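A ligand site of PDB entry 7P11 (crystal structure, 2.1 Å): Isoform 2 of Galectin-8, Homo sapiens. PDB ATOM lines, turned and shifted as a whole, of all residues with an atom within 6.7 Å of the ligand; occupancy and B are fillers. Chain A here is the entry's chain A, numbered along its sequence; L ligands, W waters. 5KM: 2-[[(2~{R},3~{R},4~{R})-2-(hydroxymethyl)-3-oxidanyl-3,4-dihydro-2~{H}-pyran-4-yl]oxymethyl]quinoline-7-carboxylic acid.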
ATOM      1  N   PRO A  12     -20.196 -35.132  -5.219  1.00  0.00           N
ATOM      2  CA  PRO A  12     -21.538 -35.069  -5.776  1.00  0.00           C
ATOM      3  C   PRO A  12     -21.920 -36.267  -6.666  1.00  0.00           C
ATOM      4  O   PRO A  12     -21.097 -36.764  -7.416  1.00  0.00           O
ATOM      5  CB  PRO A  12     -21.499 -33.807  -6.657  1.00  0.00           C
ATOM      6  CG  PRO A  12     -20.057 -33.659  -7.042  1.00  0.00           C
ATOM      7  CD  PRO A  12     -19.341 -34.084  -5.773  1.00  0.00           C
ATOM      8  N   ARG A  39     -24.426 -27.851   5.162  1.00  0.00           N
ATOM      9  CA  ARG A  39     -25.638 -28.059   4.326  1.00  0.00           C
ATOM     10  C   ARG A  39     -25.401 -29.226   3.358  1.00  0.00           C
ATOM     11  O   ARG A  39     -24.239 -29.697   3.210  1.00  0.00           O
ATOM     12  CB  ARG A  39     -25.969 -26.758   3.563  1.00  0.00           C
ATOM     13  CG  ARG A  39     -24.803 -26.164   2.789  1.00  0.00           C
ATOM     14  CD  ARG A  39     -25.336 -24.993   1.997  1.00  0.00           C
ATOM     15  NE  ARG A  39     -26.083 -25.444   0.815  1.00  0.00           N
ATOM     16  CZ  ARG A  39     -26.842 -24.677   0.024  1.00  0.00           C
ATOM     17  NH1 ARG A  39     -26.993 -23.394   0.282  1.00  0.00           N
ATOM     18  NH2 ARG A  39     -27.446 -25.204  -1.008  1.00  0.00           N
ATOM     19  N   PHE A  40     -26.467 -29.718   2.754  1.00  0.00           N
ATOM     20  CA  PHE A  40     -26.443 -30.637   1.594  1.00  0.00           C
ATOM     21  C   PHE A  40     -27.746 -30.440   0.826  1.00  0.00           C
ATOM     22  O   PHE A  40     -28.674 -29.846   1.370  1.00  0.00           O
ATOM     23  CB  PHE A  40     -26.188 -32.084   2.033  1.00  0.00           C
ATOM     24  CG  PHE A  40     -27.380 -32.822   2.572  1.00  0.00           C
ATOM     25  CD1 PHE A  40     -28.253 -33.471   1.724  1.00  0.00           C
ATOM     26  CD2 PHE A  40     -27.575 -32.937   3.926  1.00  0.00           C
ATOM     27  CE1 PHE A  40     -29.317 -34.213   2.232  1.00  0.00           C
ATOM     28  CE2 PHE A  40     -28.648 -33.663   4.434  1.00  0.00           C
ATOM     29  CZ  PHE A  40     -29.510 -34.319   3.592  1.00  0.00           C
ATOM     30  N   GLN A  41     -27.799 -30.884  -0.417  1.00  0.00           N
ATOM     31  CA  GLN A  41     -29.060 -30.690  -1.185  1.00  0.00           C
ATOM     32  C   GLN A  41     -29.372 -31.947  -1.995  1.00  0.00           C
ATOM     33  O   GLN A  41     -28.428 -32.654  -2.398  1.00  0.00           O
ATOM     34  CB  GLN A  41     -28.974 -29.455  -2.069  1.00  0.00           C
ATOM     35  CG  GLN A  41     -27.828 -29.468  -3.057  1.00  0.00           C
ATOM     36  CD  GLN A  41     -27.421 -28.047  -3.376  1.00  0.00           C
ATOM     37  OE1 GLN A  41     -26.813 -27.352  -2.550  1.00  0.00           O
ATOM     38  NE2 GLN A  41     -27.766 -27.618  -4.588  1.00  0.00           N
ATOM     39  N   ASP A  43     -31.527 -32.266  -5.476  1.00  0.00           N
ATOM     40  CA  ASP A  43     -32.081 -31.461  -6.603  1.00  0.00           C
ATOM     41  C   ASP A  43     -32.705 -32.394  -7.655  1.00  0.00           C
ATOM     42  O   ASP A  43     -32.035 -33.277  -8.188  1.00  0.00           O
ATOM     43  CB  ASP A  43     -30.996 -30.606  -7.235  1.00  0.00           C
ATOM     44  CG  ASP A  43     -30.422 -29.591  -6.252  1.00  0.00           C
ATOM     45  OD1 ASP A  43     -31.096 -29.381  -5.225  1.00  0.00           O
ATOM     46  OD2 ASP A  43     -29.326 -29.043  -6.530  1.00  0.00           O
ATOM     47  N   ARG A  53     -26.586 -23.571 -15.639  1.00  0.00           N
ATOM     48  CA  ARG A  53     -27.004 -24.609 -14.663  1.00  0.00           C
ATOM     49  C   ARG A  53     -28.433 -25.074 -14.988  1.00  0.00           C
ATOM     50  O   ARG A  53     -29.324 -24.228 -15.211  1.00  0.00           O
ATOM     51  CB  ARG A  53     -26.885 -24.053 -13.238  1.00  0.00           C
ATOM     52  CG  ARG A  53     -27.012 -25.128 -12.167  1.00  0.00           C
ATOM     53  CD  ARG A  53     -26.628 -24.594 -10.802  1.00  0.00           C
ATOM     54  NE  ARG A  53     -27.124 -25.429  -9.712  1.00  0.00           N
ATOM     55  CZ  ARG A  53     -27.152 -25.061  -8.416  1.00  0.00           C
ATOM     56  NH1 ARG A  53     -26.719 -23.866  -8.050  1.00  0.00           N
ATOM     57  NH2 ARG A  53     -27.631 -25.896  -7.500  1.00  0.00           N
ATOM     58  N   HIS A  59     -35.423 -28.161  -5.138  1.00  0.00           N
ATOM     59  CA  HIS A  59     -34.230 -28.028  -4.287  1.00  0.00           C
ATOM     60  C   HIS A  59     -34.679 -28.318  -2.871  1.00  0.00           C
ATOM     61  O   HIS A  59     -35.439 -27.522  -2.340  1.00  0.00           O
ATOM     62  CB  HIS A  59     -33.681 -26.619  -4.462  1.00  0.00           C
ATOM     63  CG  HIS A  59     -32.493 -26.241  -3.654  1.00  0.00           C
ATOM     64  ND1 HIS A  59     -31.237 -26.761  -3.880  1.00  0.00           N
ATOM     65  CD2 HIS A  59     -32.341 -25.271  -2.731  1.00  0.00           C
ATOM     66  CE1 HIS A  59     -30.366 -26.154  -3.084  1.00  0.00           C
ATOM     67  NE2 HIS A  59     -31.016 -25.236  -2.374  1.00  0.00           N
ATOM     68  N   ASN A  61     -32.884 -28.635   0.610  1.00  0.00           N
ATOM     69  CA  ASN A  61     -31.579 -28.167   1.110  1.00  0.00           C
ATOM     70  C   ASN A  61     -31.598 -28.071   2.639  1.00  0.00           C
ATOM     71  O   ASN A  61     -31.823 -27.005   3.171  1.00  0.00           O
ATOM     72  CB  ASN A  61     -31.245 -26.859   0.427  1.00  0.00           C
ATOM     73  CG  ASN A  61     -30.028 -26.156   0.993  1.00  0.00           C
ATOM     74  OD1 ASN A  61     -30.009 -24.923   1.047  1.00  0.00           O
ATOM     75  ND2 ASN A  61     -29.019 -26.941   1.352  1.00  0.00           N
ATOM     76  N   ARG A  63     -30.057 -27.337   6.112  1.00  0.00           N
ATOM     77  CA  ARG A  63     -29.005 -26.433   6.663  1.00  0.00           C
ATOM     78  C   ARG A  63     -28.879 -26.699   8.165  1.00  0.00           C
ATOM     79  O   ARG A  63     -29.905 -27.050   8.789  1.00  0.00           O
ATOM     80  CB  ARG A  63     -29.329 -24.968   6.361  1.00  0.00           C
ATOM     81  CG  ARG A  63     -29.326 -24.658   4.872  1.00  0.00           C
ATOM     82  CD  ARG A  63     -29.653 -23.202   4.504  1.00  0.00           C
ATOM     83  NE  ARG A  63     -29.829 -23.080   3.052  1.00  0.00           N
ATOM     84  CZ  ARG A  63     -29.924 -21.946   2.347  1.00  0.00           C
ATOM     85  NH1 ARG A  63     -29.845 -20.779   2.978  1.00  0.00           N
ATOM     86  NH2 ARG A  63     -30.098 -21.971   1.042  1.00  0.00           N
ATOM     87  N   VAL A  71     -34.368 -25.439   3.550  1.00  0.00           N
ATOM     88  CA  VAL A  71     -34.786 -24.487   2.504  1.00  0.00           C
ATOM     89  C   VAL A  71     -35.197 -25.327   1.308  1.00  0.00           C
ATOM     90  O   VAL A  71     -34.466 -26.258   0.986  1.00  0.00           O
ATOM     91  CB  VAL A  71     -33.682 -23.477   2.176  1.00  0.00           C
ATOM     92  CG1 VAL A  71     -34.059 -22.578   0.988  1.00  0.00           C
ATOM     93  CG2 VAL A  71     -33.329 -22.641   3.393  1.00  0.00           C
ATOM     94  N   CYS A  72     -36.388 -25.065   0.753  1.00  0.00           N
ATOM     95  CA  CYS A  72     -36.848 -25.611  -0.543  1.00  0.00           C
ATOM     96  C   CYS A  72     -37.086 -24.462  -1.498  1.00  0.00           C
ATOM     97  O   CYS A  72     -37.532 -23.419  -1.042  1.00  0.00           O
ATOM     98  CB  CYS A  72     -38.114 -26.444  -0.379  1.00  0.00           C
ATOM     99  SG  CYS A  72     -37.839 -27.873   0.701  1.00  0.00           S
ATOM    100  N   ASN A  73     -36.737 -24.623  -2.763  1.00  0.00           N
ATOM    101  CA  ASN A  73     -36.873 -23.544  -3.763  1.00  0.00           C
ATOM    102  C   ASN A  73     -36.771 -24.157  -5.163  1.00  0.00           C
ATOM    103  O   ASN A  73     -36.583 -25.384  -5.271  1.00  0.00           O
ATOM    104  CB  ASN A  73     -35.857 -22.443  -3.488  1.00  0.00           C
ATOM    105  CG  ASN A  73     -36.240 -21.102  -4.103  1.00  0.00           C
ATOM    106  OD1 ASN A  73     -37.124 -21.021  -4.929  1.00  0.00           O
ATOM    107  ND2 ASN A  73     -35.524 -20.050  -3.747  1.00  0.00           N
ATOM    108  N   THR A  74     -36.926 -23.319  -6.196  1.00  0.00           N
ATOM    109  CA  THR A  74     -36.899 -23.697  -7.620  1.00  0.00           C
ATOM    110  C   THR A  74     -35.963 -22.748  -8.366  1.00  0.00           C
ATOM    111  O   THR A  74     -36.089 -21.518  -8.135  1.00  0.00           O
ATOM    112  CB  THR A  74     -38.316 -23.689  -8.184  1.00  0.00           C
ATOM    113  OG1 THR A  74     -38.995 -24.750  -7.507  1.00  0.00           O
ATOM    114  CG2 THR A  74     -38.397 -23.845  -9.694  1.00  0.00           C
ATOM    115  N   TRP A  80     -33.279 -18.242  -8.592  1.00  0.00           N
ATOM    116  CA  TRP A  80     -34.072 -18.849  -7.482  1.00  0.00           C
ATOM    117  C   TRP A  80     -35.406 -18.089  -7.288  1.00  0.00           C
ATOM    118  O   TRP A  80     -35.426 -16.877  -7.507  1.00  0.00           O
ATOM    119  CB  TRP A  80     -33.242 -18.877  -6.195  1.00  0.00           C
ATOM    120  CG  TRP A  80     -32.063 -19.790  -6.261  1.00  0.00           C
ATOM    121  CD1 TRP A  80     -30.746 -19.435  -6.385  1.00  0.00           C
ATOM    122  CD2 TRP A  80     -32.063 -21.226  -6.186  1.00  0.00           C
ATOM    123  NE1 TRP A  80     -29.937 -20.534  -6.385  1.00  0.00           N
ATOM    124  CE2 TRP A  80     -30.716 -21.649  -6.282  1.00  0.00           C
ATOM    125  CE3 TRP A  80     -33.060 -22.189  -6.045  1.00  0.00           C
ATOM    126  CZ2 TRP A  80     -30.345 -23.003  -6.220  1.00  0.00           C
ATOM    127  CZ3 TRP A  80     -32.697 -23.528  -5.984  1.00  0.00           C
ATOM    128  CH2 TRP A  80     -31.360 -23.922  -6.059  1.00  0.00           C
ATOM    129  N   GLY A  81     -36.496 -18.783  -6.950  1.00  0.00           N
ATOM    130  CA  GLY A  81     -37.790 -18.157  -6.633  1.00  0.00           C
ATOM    131  C   GLY A  81     -37.876 -17.867  -5.146  1.00  0.00           C
ATOM    132  O   GLY A  81     -36.844 -17.859  -4.500  1.00  0.00           O
ATOM    133  N   ARG A  82     -39.075 -17.683  -4.606  1.00  0.00           N
ATOM    134  CA  ARG A  82     -39.274 -17.410  -3.166  1.00  0.00           C
ATOM    135  C   ARG A  82     -38.918 -18.664  -2.353  1.00  0.00           C
ATOM    136  O   ARG A  82     -39.469 -19.737  -2.649  1.00  0.00           O
ATOM    137  CB  ARG A  82     -40.698 -16.889  -2.964  1.00  0.00           C
ATOM    138  CG  ARG A  82     -41.185 -16.996  -1.529  1.00  0.00           C
ATOM    139  CD  ARG A  82     -42.554 -16.405  -1.293  1.00  0.00           C
ATOM    140  NE  ARG A  82     -43.796 -16.991  -1.836  1.00  0.00           N
ATOM    141  CZ  ARG A  82     -44.199 -18.264  -1.773  1.00  0.00           C
ATOM    142  NH1 ARG A  82     -45.381 -18.573  -2.269  1.00  0.00           N
ATOM    143  NH2 ARG A  82     -43.461 -19.225  -1.240  1.00  0.00           N
ATOM    144  N   GLU A  83     -38.007 -18.550  -1.380  1.00  0.00           N
ATOM    145  CA  GLU A  83     -37.603 -19.684  -0.511  1.00  0.00           C
ATOM    146  C   GLU A  83     -38.791 -20.110   0.342  1.00  0.00           C
ATOM    147  O   GLU A  83     -39.567 -19.221   0.743  1.00  0.00           O
ATOM    148  CB  GLU A  83     -36.430 -19.351   0.404  1.00  0.00           C
ATOM    149  CG  GLU A  83     -35.090 -19.377  -0.305  1.00  0.00           C
ATOM    150  CD  GLU A  83     -33.903 -18.842   0.485  1.00  0.00           C
ATOM    151  OE1 GLU A  83     -34.120 -18.174   1.507  1.00  0.00           O
ATOM    152  OE2 GLU A  83     -32.763 -19.074   0.084  1.00  0.00           O
ATOM    153  N   TYR A 135     -25.601 -32.979  -3.687  1.00  0.00           N
ATOM    154  CA  TYR A 135     -24.387 -32.121  -3.531  1.00  0.00           C
ATOM    155  C   TYR A 135     -24.209 -31.775  -2.051  1.00  0.00           C
ATOM    156  O   TYR A 135     -25.212 -31.842  -1.305  1.00  0.00           O
ATOM    157  CB  TYR A 135     -24.502 -30.864  -4.393  1.00  0.00           C
ATOM    158  CG  TYR A 135     -25.011 -31.111  -5.798  1.00  0.00           C
ATOM    159  CD1 TYR A 135     -26.360 -31.276  -6.064  1.00  0.00           C
ATOM    160  CD2 TYR A 135     -24.152 -31.183  -6.883  1.00  0.00           C
ATOM    161  CE1 TYR A 135     -26.841 -31.473  -7.344  1.00  0.00           C
ATOM    162  CE2 TYR A 135     -24.610 -31.407  -8.174  1.00  0.00           C
ATOM    163  CZ  TYR A 135     -25.964 -31.541  -8.407  1.00  0.00           C
ATOM    164  OH  TYR A 135     -26.411 -31.745  -9.674  1.00  0.00           O
ATOM    165  N   GLY A 136     -22.977 -31.434  -1.643  1.00  0.00           N
ATOM    166  CA  GLY A 136     -22.644 -30.922  -0.293  1.00  0.00           C
ATOM    167  C   GLY A 136     -22.119 -32.002   0.658  1.00  0.00           C
ATOM    168  O   GLY A 136     -21.680 -33.042   0.181  1.00  0.00           O
ATOM    169  N   LYS A 137     -22.114 -31.727   1.970  1.00  0.00           N
ATOM    170  CA  LYS A 137     -21.537 -32.639   2.997  1.00  0.00           C
ATOM    171  C   LYS A 137     -22.586 -33.657   3.430  1.00  0.00           C
ATOM    172  O   LYS A 137     -23.372 -33.391   4.347  1.00  0.00           O
ATOM    173  CB  LYS A 137     -20.983 -31.853   4.199  1.00  0.00           C
ATOM    174  CG  LYS A 137     -19.966 -30.787   3.805  1.00  0.00           C
ATOM    175  CD  LYS A 137     -18.743 -30.696   4.671  1.00  0.00           C
ATOM    176  CE  LYS A 137     -17.635 -29.962   3.941  1.00  0.00           C
ATOM    177  NZ  LYS A 137     -16.827 -29.156   4.870  1.00  0.00           N
HETATM  178  C1  5KM L   1     -30.585 -21.165  -2.497  1.00  0.00           C
HETATM  179  C2  5KM L   1     -29.626 -22.340  -2.518  1.00  0.00           C
HETATM  180  C3  5KM L   1     -28.260 -21.841  -2.960  1.00  0.00           C
HETATM  181  C4  5KM L   1     -26.066 -22.608  -3.417  1.00  0.00           C
HETATM  182  C5  5KM L   1     -25.313 -23.882  -3.727  1.00  0.00           C
HETATM  183  C6  5KM L   1     -23.921 -25.602  -3.057  1.00  0.00           C
HETATM  184  C7  5KM L   1     -23.975 -26.246  -4.432  1.00  0.00           C
HETATM  185  O4  5KM L   1     -22.352 -27.727  -0.136  1.00  0.00           O
HETATM  186  C11 5KM L   1     -21.790 -27.849  -1.227  1.00  0.00           C
HETATM  187  O3  5KM L   1     -20.581 -28.399  -1.352  1.00  0.00           O
HETATM  188  C10 5KM L   1     -22.532 -27.344  -2.389  1.00  0.00           C
HETATM  189  C12 5KM L   1     -23.193 -26.184  -2.065  1.00  0.00           C
HETATM  190  N   5KM L   1     -24.570 -24.456  -2.757  1.00  0.00           N
HETATM  191  C9  5KM L   1     -22.544 -27.982  -3.635  1.00  0.00           C
HETATM  192  C8  5KM L   1     -23.281 -27.433  -4.708  1.00  0.00           C
HETATM  193  C13 5KM L   1     -24.751 -25.617  -5.371  1.00  0.00           C
HETATM  194  C14 5KM L   1     -25.415 -24.451  -4.993  1.00  0.00           C
HETATM  195  O2  5KM L   1     -27.365 -22.945  -2.920  1.00  0.00           O
HETATM  196  O1  5KM L   1     -29.568 -23.082  -1.279  1.00  0.00           O
HETATM  197  C15 5KM L   1     -27.825 -20.661  -2.093  1.00  0.00           C
HETATM  198  C16 5KM L   1     -28.717 -19.876  -1.504  1.00  0.00           C
HETATM  199  O5  5KM L   1     -30.138 -20.128  -1.618  1.00  0.00           O
HETATM  200  C   5KM L   1     -31.965 -21.579  -2.045  1.00  0.00           C
HETATM  201  O   5KM L   1     -32.831 -20.546  -2.418  1.00  0.00           O
HETATM  202  O   HOH W   1     -27.213 -18.869  -4.586  1.00  0.00           O
HETATM  203  O   HOH W   2     -25.514 -28.111  -0.106  1.00  0.00           O
HETATM  204  O   HOH W   3     -19.105 -29.747   1.018  1.00  0.00           O
HETATM  205  O   HOH W   4     -21.175 -28.492   2.099  1.00  0.00           O
HETATM  206  O   HOH W   5     -26.973 -21.733  -6.320  1.00  0.00           O
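The guanidinium group (NH2) of Arg 63 sits at hydrogen-bond distance from an oxygen (O1) of the ligand (2.6 Å). NE2 of His 59 lies within hydrogen-bond range of O1 of the ligand. The side-chain carboxylate (OE2) of Glu 83 lies within hydrogen-bond range of an oxygen (O) of the ligand, 2.9 Å away. An oxygen (O2) of the ligand sits at hydrogen-bond distance from the guanidinium group (NH2) of Arg 39, 3.0 Å away. The side-chain amide oxygen of Asn 61 sits at hydrogen-bond distance from an oxygen (O1) of the ligand, 3.0 Å away. The side-chain amide nitrogen of Asn 73 is in hydrogen-bond range of an oxygen (O) of the ligand, 3.0 Å away.
The side-chain amide oxygen (OD1) of Asn 61 sits at hydrogen-bond distance from the guanidinium group (NE) of Arg 63 (2.7 Å). OD1 of Asp 43 is in hydrogen-bond range of ND1 of His 59, at 2.9 Å. The guanidinium group of Arg 39 lies within hydrogen-bond range of the side-chain amide oxygen of Asn 61, 3.3 Å away. The backbone carbonyl oxygen (O) of Arg 39 lies within hydrogen-bond range of the backbone NH (N) of Lys 137 (3.2 Å). The side-chain amide nitrogen (ND2) of Asn 61 lies within hydrogen-bond range of the backbone carbonyl oxygen (O) of Phe 40. NH2 of Arg 53 sits close to NE2 of Gln 41 (3.4 Å). The guanidinium group (NH2) of Arg 53 is in salt-bridge range of the side-chain carboxylate (OD2) of Asp 43 (3.7 Å). The backbone NH of Gln 41 is in hydrogen-bond range of the backbone carbonyl oxygen of Tyr 135, 2.9 Å away.
Gln 41 touches the ligand (OE1 to C6, 3.4 Å). Arg 53 touches the ligand. Val 71 touches the ligand (CG1 to C, 3.8 Å). Trp 80 touches the ligand. CB of Tyr 135 touches C9 of the ligand, 3.6 Å away. Gly 136 touches the ligand. 12 residues have an atom within 4 Å of the ligand: Arg 39, Gln 41, Arg 53, His 59, Asn 61, Arg 63, Val 71, Asn 73, Trp 80, Glu 83, Tyr 135 and Gly 136. The nearest printed residue that does not touch the ligand is Lys 137 (4.5 Å).
Water W4 lies within hydrogen-bond range of an oxygen (O4) of the ligand (2.6 Å), the backbone NH of Lys 137 (3.4 Å) and the backbone carbonyl oxygen of Arg 39 (3.5 Å). Water W5 bridges the guanidinium group (NH1) of Arg 53 (2.8 Å) and the indole nitrogen (NE1) of Trp 80 (3.2 Å). Water W2 lies within hydrogen-bond range of OE1 of Gln 41 (2.9 Å), NE of Arg 39 (2.9 Å), O4 of the ligand (3.2 Å) and N of Phe 40 (3.4 Å).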
